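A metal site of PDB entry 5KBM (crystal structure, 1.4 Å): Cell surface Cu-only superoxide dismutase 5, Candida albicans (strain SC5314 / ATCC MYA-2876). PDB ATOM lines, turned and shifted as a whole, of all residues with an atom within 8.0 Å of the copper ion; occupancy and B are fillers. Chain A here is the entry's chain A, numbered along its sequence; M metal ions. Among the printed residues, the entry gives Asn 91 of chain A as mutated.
NE2 of His 71 sits close to ND1 of His 53, at 3.1 Å.
The backbone carbonyl oxygen (O) of Pro 51 lies within hydrogen-bond range of the backbone NH (N) of His 131 (2.8 Å).
The backbone carbonyl oxygen (O) of Gly 135 lies within hydrogen-bond range of a ring nitrogen (ND1) of His 131 (2.8 Å).
The backbone carbonyl oxygen (O) of Glu 69 lies within hydrogen-bond range of a ring nitrogen (ND1) of His 55 (2.8 Å).
The backbone carbonyl oxygen of His 53 sits at hydrogen-bond distance from the backbone NH of Val 129, 3.1 Å away.
The backbone NH of His 55 sits at hydrogen-bond distance from the backbone carbonyl oxygen of Ser 127 (2.8 Å).
O of Asn 70 lies close to ND1 of His 55 (3.3 Å).
His 71 touches the copper ion.
Val 129 touches the copper ion (CB to CU, 3.9 Å).
Within 4 Å of the copper ion: His 53, His 55, His 71, Val 129 and His 131.
The copper ion is bound by NE2 of His 55 (2.0 Å).
The copper ion is bound by a ring nitrogen (ND1) of His 53, 2.0 Å away.
The copper ion is bound by NE2 of His 131 (2.0 Å).
The copper ion has three donor atoms within binding distance.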
ATOM      1  N   PRO A  51      -7.781  -4.976 -21.868  1.00  0.00           N
ATOM      2  CA  PRO A  51      -7.462  -3.556 -22.009  1.00  0.00           C
ATOM      3  C   PRO A  51      -7.536  -3.141 -23.462  1.00  0.00           C
ATOM      4  O   PRO A  51      -7.284  -3.922 -24.395  1.00  0.00           O
ATOM      5  CB  PRO A  51      -6.039  -3.446 -21.462  1.00  0.00           C
ATOM      6  CG  PRO A  51      -5.840  -4.648 -20.591  1.00  0.00           C
ATOM      7  CD  PRO A  51      -6.696  -5.735 -21.219  1.00  0.00           C
ATOM      8  N   TYR A  52      -7.922  -1.888 -23.657  1.00  0.00           N
ATOM      9  CA  TYR A  52      -7.898  -1.273 -24.957  1.00  0.00           C
ATOM     10  C   TYR A  52      -7.539   0.188 -24.783  1.00  0.00           C
ATOM     11  O   TYR A  52      -7.939   0.813 -23.780  1.00  0.00           O
ATOM     12  CB  TYR A  52      -9.208  -1.465 -25.716  1.00  0.00           C
ATOM     13  CG  TYR A  52     -10.427  -0.784 -25.129  1.00  0.00           C
ATOM     14  CD1 TYR A  52     -11.028  -1.235 -23.971  1.00  0.00           C
ATOM     15  CD2 TYR A  52     -11.015   0.292 -25.788  1.00  0.00           C
ATOM     16  CE1 TYR A  52     -12.160  -0.628 -23.471  1.00  0.00           C
ATOM     17  CE2 TYR A  52     -12.146   0.897 -25.305  1.00  0.00           C
ATOM     18  CZ  TYR A  52     -12.710   0.431 -24.160  1.00  0.00           C
ATOM     19  OH  TYR A  52     -13.841   1.078 -23.676  1.00  0.00           O
ATOM     20  N   HIS A  53      -6.789   0.723 -25.732  1.00  0.00           N
ATOM     21  CA  HIS A  53      -6.231   2.062 -25.628  1.00  0.00           C
ATOM     22  C   HIS A  53      -6.112   2.664 -27.022  1.00  0.00           C
ATOM     23  O   HIS A  53      -6.010   1.965 -28.027  1.00  0.00           O
ATOM     24  CB  HIS A  53      -4.817   2.040 -25.047  1.00  0.00           C
ATOM     25  CG  HIS A  53      -4.597   0.968 -24.033  1.00  0.00           C
ATOM     26  ND1 HIS A  53      -3.991  -0.230 -24.350  1.00  0.00           N
ATOM     27  CD2 HIS A  53      -4.923   0.899 -22.728  1.00  0.00           C
ATOM     28  CE1 HIS A  53      -3.923  -0.980 -23.264  1.00  0.00           C
ATOM     29  NE2 HIS A  53      -4.492  -0.321 -22.270  1.00  0.00           N
ATOM     30  N   VAL A  54      -6.089   3.986 -27.045  1.00  0.00           N
ATOM     31  CA  VAL A  54      -5.643   4.706 -28.235  1.00  0.00           C
ATOM     32  C   VAL A  54      -4.121   4.678 -28.245  1.00  0.00           C
ATOM     33  O   VAL A  54      -3.483   5.017 -27.237  1.00  0.00           O
ATOM     34  CB  VAL A  54      -6.179   6.146 -28.210  1.00  0.00           C
ATOM     35  CG1 VAL A  54      -5.767   6.896 -29.490  1.00  0.00           C
ATOM     36  CG2 VAL A  54      -7.687   6.160 -28.051  1.00  0.00           C
ATOM     37  N   HIS A  55      -3.547   4.261 -29.374  1.00  0.00           N
ATOM     38  CA  HIS A  55      -2.105   4.208 -29.582  1.00  0.00           C
ATOM     39  C   HIS A  55      -1.684   5.320 -30.539  1.00  0.00           C
ATOM     40  O   HIS A  55      -2.508   5.987 -31.163  1.00  0.00           O
ATOM     41  CB  HIS A  55      -1.670   2.817 -30.096  1.00  0.00           C
ATOM     42  CG  HIS A  55      -1.683   1.752 -29.035  1.00  0.00           C
ATOM     43  ND1 HIS A  55      -0.550   1.059 -28.665  1.00  0.00           N
ATOM     44  CD2 HIS A  55      -2.694   1.275 -28.254  1.00  0.00           C
ATOM     45  CE1 HIS A  55      -0.860   0.201 -27.701  1.00  0.00           C
ATOM     46  NE2 HIS A  55      -2.157   0.313 -27.445  1.00  0.00           N
ATOM     47  N   CYS A  65      -0.388  -4.995 -35.422  1.00  0.00           N
ATOM     48  CA  CYS A  65      -0.771  -4.118 -34.322  1.00  0.00           C
ATOM     49  C   CYS A  65       0.421  -3.600 -33.529  1.00  0.00           C
ATOM     50  O   CYS A  65       0.299  -2.585 -32.847  1.00  0.00           O
ATOM     51  CB  CYS A  65      -1.766  -4.832 -33.397  1.00  0.00           C
ATOM     52  SG  CYS A  65      -3.344  -5.308 -34.240  1.00  0.00           S
ATOM     53  N   THR A  68       1.591   0.137 -34.236  1.00  0.00           N
ATOM     54  CA  THR A  68       0.951   1.309 -33.638  1.00  0.00           C
ATOM     55  C   THR A  68       1.774   1.886 -32.503  1.00  0.00           C
ATOM     56  O   THR A  68       1.430   2.967 -32.022  1.00  0.00           O
ATOM     57  CB  THR A  68      -0.454   0.969 -33.130  1.00  0.00           C
ATOM     58  OG1 THR A  68      -0.379   0.044 -32.026  1.00  0.00           O
ATOM     59  CG2 THR A  68      -1.332   0.403 -34.214  1.00  0.00           C
ATOM     60  N   GLU A  69       2.814   1.180 -32.052  1.00  0.00           N
ATOM     61  CA  GLU A  69       3.719   1.661 -31.013  1.00  0.00           C
ATOM     62  C   GLU A  69       2.985   1.857 -29.695  1.00  0.00           C
ATOM     63  O   GLU A  69       2.178   1.002 -29.307  1.00  0.00           O
ATOM     64  CB  GLU A  69       4.476   2.916 -31.487  1.00  0.00           C
ATOM     65  CG  GLU A  69       5.425   2.629 -32.678  1.00  0.00           C
ATOM     66  CD  GLU A  69       6.343   3.796 -33.055  1.00  0.00           C
ATOM     67  OE1 GLU A  69       6.400   4.809 -32.315  1.00  0.00           O
ATOM     68  OE2 GLU A  69       7.022   3.694 -34.098  1.00  0.00           O
ATOM     69  N   ASN A  70       3.230   2.954 -28.994  1.00  0.00           N
ATOM     70  CA  ASN A  70       2.837   3.046 -27.594  1.00  0.00           C
ATOM     71  C   ASN A  70       1.474   3.707 -27.428  1.00  0.00           C
ATOM     72  O   ASN A  70       0.805   4.094 -28.386  1.00  0.00           O
ATOM     73  CB  ASN A  70       3.905   3.801 -26.791  1.00  0.00           C
ATOM     74  CG  ASN A  70       5.235   3.091 -26.761  1.00  0.00           C
ATOM     75  OD1 ASN A  70       5.309   1.848 -26.792  1.00  0.00           O
ATOM     76  ND2 ASN A  70       6.307   3.879 -26.723  1.00  0.00           N
ATOM     77  N   HIS A  71       1.066   3.847 -26.170  1.00  0.00           N
ATOM     78  CA  HIS A  71      -0.191   4.514 -25.854  1.00  0.00           C
ATOM     79  C   HIS A  71      -0.102   5.988 -26.194  1.00  0.00           C
ATOM     80  O   HIS A  71       0.947   6.625 -26.056  1.00  0.00           O
ATOM     81  CB  HIS A  71      -0.491   4.402 -24.371  1.00  0.00           C
ATOM     82  CG  HIS A  71      -0.805   3.010 -23.918  1.00  0.00           C
ATOM     83  ND1 HIS A  71      -1.241   2.742 -22.633  1.00  0.00           N
ATOM     84  CD2 HIS A  71      -0.757   1.820 -24.560  1.00  0.00           C
ATOM     85  CE1 HIS A  71      -1.445   1.442 -22.514  1.00  0.00           C
ATOM     86  NE2 HIS A  71      -1.158   0.863 -23.669  1.00  0.00           N
ATOM     87  N   PHE A  72      -1.221   6.546 -26.622  1.00  0.00           N
ATOM     88  CA  PHE A  72      -1.350   7.990 -26.763  1.00  0.00           C
ATOM     89  C   PHE A  72      -1.505   8.560 -25.355  1.00  0.00           C
ATOM     90  O   PHE A  72      -2.614   8.784 -24.855  1.00  0.00           O
ATOM     91  CB  PHE A  72      -2.544   8.313 -27.648  1.00  0.00           C
ATOM     92  CG  PHE A  72      -2.757   9.774 -27.881  1.00  0.00           C
ATOM     93  CD1 PHE A  72      -1.815  10.538 -28.548  1.00  0.00           C
ATOM     94  CD2 PHE A  72      -3.913  10.392 -27.432  1.00  0.00           C
ATOM     95  CE1 PHE A  72      -2.036  11.883 -28.762  1.00  0.00           C
ATOM     96  CE2 PHE A  72      -4.134  11.712 -27.642  1.00  0.00           C
ATOM     97  CZ  PHE A  72      -3.201  12.473 -28.298  1.00  0.00           C
ATOM     98  N   GLU A  88      -3.717   7.480 -18.296  1.00  0.00           N
ATOM     99  CA  GLU A  88      -3.305   7.915 -19.622  1.00  0.00           C
ATOM    100  C   GLU A  88      -4.550   8.314 -20.428  1.00  0.00           C
ATOM    101  O   GLU A  88      -5.600   7.670 -20.337  1.00  0.00           O
ATOM    102  CB  GLU A  88      -2.561   6.796 -20.346  1.00  0.00           C
ATOM    103  CG  GLU A  88      -1.458   6.071 -19.523  1.00  0.00           C
ATOM    104  CD  GLU A  88      -1.203   4.657 -20.005  1.00  0.00           C
ATOM    105  OE1 GLU A  88      -1.937   4.192 -20.907  1.00  0.00           O
ATOM    106  OE2 GLU A  88      -0.269   4.000 -19.495  1.00  0.00           O
ATOM    107  N   GLY A  90      -5.155   8.037 -23.605  1.00  0.00           N
ATOM    108  CA  GLY A  90      -5.580   6.930 -24.422  1.00  0.00           C
ATOM    109  C   GLY A  90      -5.983   5.703 -23.647  1.00  0.00           C
ATOM    110  O   GLY A  90      -6.429   4.737 -24.268  1.00  0.00           O
ATOM    111  N   ASN A  91      -5.901   5.727 -22.309  1.00  0.00           N
ATOM    112  CA  ASN A  91      -6.219   4.524 -21.529  1.00  0.00           C
ATOM    113  C   ASN A  91      -7.723   4.487 -21.263  1.00  0.00           C
ATOM    114  O   ASN A  91      -8.202   4.674 -20.153  1.00  0.00           O
ATOM    115  CB  ASN A  91      -5.421   4.413 -20.243  1.00  0.00           C
ATOM    116  CG  ASN A  91      -5.567   3.051 -19.607  1.00  0.00           C
ATOM    117  OD1 ASN A  91      -6.272   2.186 -20.126  1.00  0.00           O
ATOM    118  ND2 ASN A  91      -4.894   2.836 -18.489  1.00  0.00           N
ATOM    119  N   SER A 127      -5.044   5.137 -33.584  1.00  0.00           N
ATOM    120  CA  SER A 127      -5.463   3.760 -33.657  1.00  0.00           C
ATOM    121  C   SER A 127      -5.927   3.309 -32.293  1.00  0.00           C
ATOM    122  O   SER A 127      -5.618   3.932 -31.273  1.00  0.00           O
ATOM    123  CB  SER A 127      -4.317   2.834 -34.132  1.00  0.00           C
ATOM    124  OG  SER A 127      -3.248   2.875 -33.219  1.00  0.00           O
ATOM    125  N   ILE A 128      -6.682   2.224 -32.286  1.00  0.00           N
ATOM    126  CA  ILE A 128      -7.048   1.543 -31.046  1.00  0.00           C
ATOM    127  C   ILE A 128      -6.550   0.113 -31.122  1.00  0.00           C
ATOM    128  O   ILE A 128      -6.693  -0.542 -32.162  1.00  0.00           O
ATOM    129  CB  ILE A 128      -8.569   1.561 -30.824  1.00  0.00           C
ATOM    130  CG1 ILE A 128      -9.079   2.996 -30.773  1.00  0.00           C
ATOM    131  CG2 ILE A 128      -8.908   0.824 -29.568  1.00  0.00           C
ATOM    132  CD1 ILE A 128     -10.529   3.136 -30.782  1.00  0.00           C
ATOM    133  N   VAL A 129      -5.958  -0.359 -30.026  1.00  0.00           N
ATOM    134  CA  VAL A 129      -5.507  -1.737 -29.902  1.00  0.00           C
ATOM    135  C   VAL A 129      -6.295  -2.386 -28.784  1.00  0.00           C
ATOM    136  O   VAL A 129      -6.482  -1.782 -27.711  1.00  0.00           O
ATOM    137  CB  VAL A 129      -3.992  -1.832 -29.629  1.00  0.00           C
ATOM    138  CG1 VAL A 129      -3.550  -3.273 -29.411  1.00  0.00           C
ATOM    139  CG2 VAL A 129      -3.186  -1.197 -30.790  1.00  0.00           C
ATOM    140  N   ILE A 130      -6.770  -3.602 -29.013  1.00  0.00           N
ATOM    141  CA  ILE A 130      -7.370  -4.450 -27.991  1.00  0.00           C
ATOM    142  C   ILE A 130      -6.335  -5.495 -27.614  1.00  0.00           C
ATOM    143  O   ILE A 130      -5.785  -6.175 -28.483  1.00  0.00           O
ATOM    144  CB  ILE A 130      -8.667  -5.091 -28.498  1.00  0.00           C
ATOM    145  CG1 ILE A 130      -9.666  -3.985 -28.880  1.00  0.00           C
ATOM    146  CG2 ILE A 130      -9.256  -6.007 -27.431  1.00  0.00           C
ATOM    147  CD1 ILE A 130     -10.883  -4.487 -29.555  1.00  0.00           C
ATOM    148  N   HIS A 131      -6.072  -5.638 -26.306  1.00  0.00           N
ATOM    149  CA  HIS A 131      -5.072  -6.554 -25.790  1.00  0.00           C
ATOM    150  C   HIS A 131      -5.730  -7.690 -25.029  1.00  0.00           C
ATOM    151  O   HIS A 131      -6.787  -7.520 -24.407  1.00  0.00           O
ATOM    152  CB  HIS A 131      -4.137  -5.863 -24.787  1.00  0.00           C
ATOM    153  CG  HIS A 131      -3.423  -4.678 -25.327  1.00  0.00           C
ATOM    154  ND1 HIS A 131      -2.072  -4.664 -25.558  1.00  0.00           N
ATOM    155  CD2 HIS A 131      -3.861  -3.435 -25.642  1.00  0.00           C
ATOM    156  CE1 HIS A 131      -1.701  -3.484 -26.002  1.00  0.00           C
ATOM    157  NE2 HIS A 131      -2.771  -2.717 -26.078  1.00  0.00           N
ATOM    158  N   GLY A 135      -1.150  -8.443 -22.124  1.00  0.00           N
ATOM    159  CA  GLY A 135      -0.541  -7.432 -22.967  1.00  0.00           C
ATOM    160  C   GLY A 135      -0.501  -7.759 -24.447  1.00  0.00           C
ATOM    161  O   GLY A 135      -0.321  -6.846 -25.244  1.00  0.00           O
ATOM    162  N   THR A 136      -0.605  -9.038 -24.830  1.00  0.00           N
ATOM    163  CA  THR A 136      -0.550  -9.378 -26.249  1.00  0.00           C
ATOM    164  C   THR A 136      -1.600  -8.599 -27.038  1.00  0.00           C
ATOM    165  O   THR A 136      -2.744  -8.474 -26.605  1.00  0.00           O
ATOM    166  CB  THR A 136      -0.829 -10.876 -26.427  1.00  0.00           C
ATOM    167  OG1 THR A 136       0.141 -11.638 -25.701  1.00  0.00           O
ATOM    168  CG2 THR A 136      -0.788 -11.278 -27.915  1.00  0.00           C
ATOM    169  N   ARG A 137      -1.211  -8.098 -28.205  1.00  0.00           N
ATOM    170  CA  ARG A 137      -2.114  -7.327 -29.049  1.00  0.00           C
ATOM    171  C   ARG A 137      -2.926  -8.286 -29.917  1.00  0.00           C
ATOM    172  O   ARG A 137      -2.348  -9.056 -30.691  1.00  0.00           O
ATOM    173  CB  ARG A 137      -1.342  -6.304 -29.877  1.00  0.00           C
ATOM    174  CG  ARG A 137      -0.473  -5.386 -29.004  1.00  0.00           C
ATOM    175  CD  ARG A 137       0.231  -4.274 -29.728  1.00  0.00           C
ATOM    176  NE  ARG A 137       0.941  -3.454 -28.752  1.00  0.00           N
ATOM    177  CZ  ARG A 137       1.447  -2.249 -28.993  1.00  0.00           C
ATOM    178  NH1 ARG A 137       1.334  -1.702 -30.186  1.00  0.00           N
ATOM    179  NH2 ARG A 137       2.067  -1.589 -28.023  1.00  0.00           N
ATOM    180  N   ASN A 139      -6.226  -7.371 -31.817  1.00  0.00           N
ATOM    181  CA  ASN A 139      -6.674  -6.713 -33.023  1.00  0.00           C
ATOM    182  C   ASN A 139      -6.561  -5.220 -32.807  1.00  0.00           C
ATOM    183  O   ASN A 139      -6.397  -4.742 -31.677  1.00  0.00           O
ATOM    184  CB  ASN A 139      -8.102  -7.140 -33.354  1.00  0.00           C
ATOM    185  CG  ASN A 139      -8.467  -6.966 -34.799  1.00  0.00           C
ATOM    186  OD1 ASN A 139      -7.745  -6.345 -35.598  1.00  0.00           O
ATOM    187  ND2 ASN A 139      -9.637  -7.489 -35.150  1.00  0.00           N
HETATM  188 CU    CU M   1      -3.010  -0.684 -26.002  1.00  0.00          CU
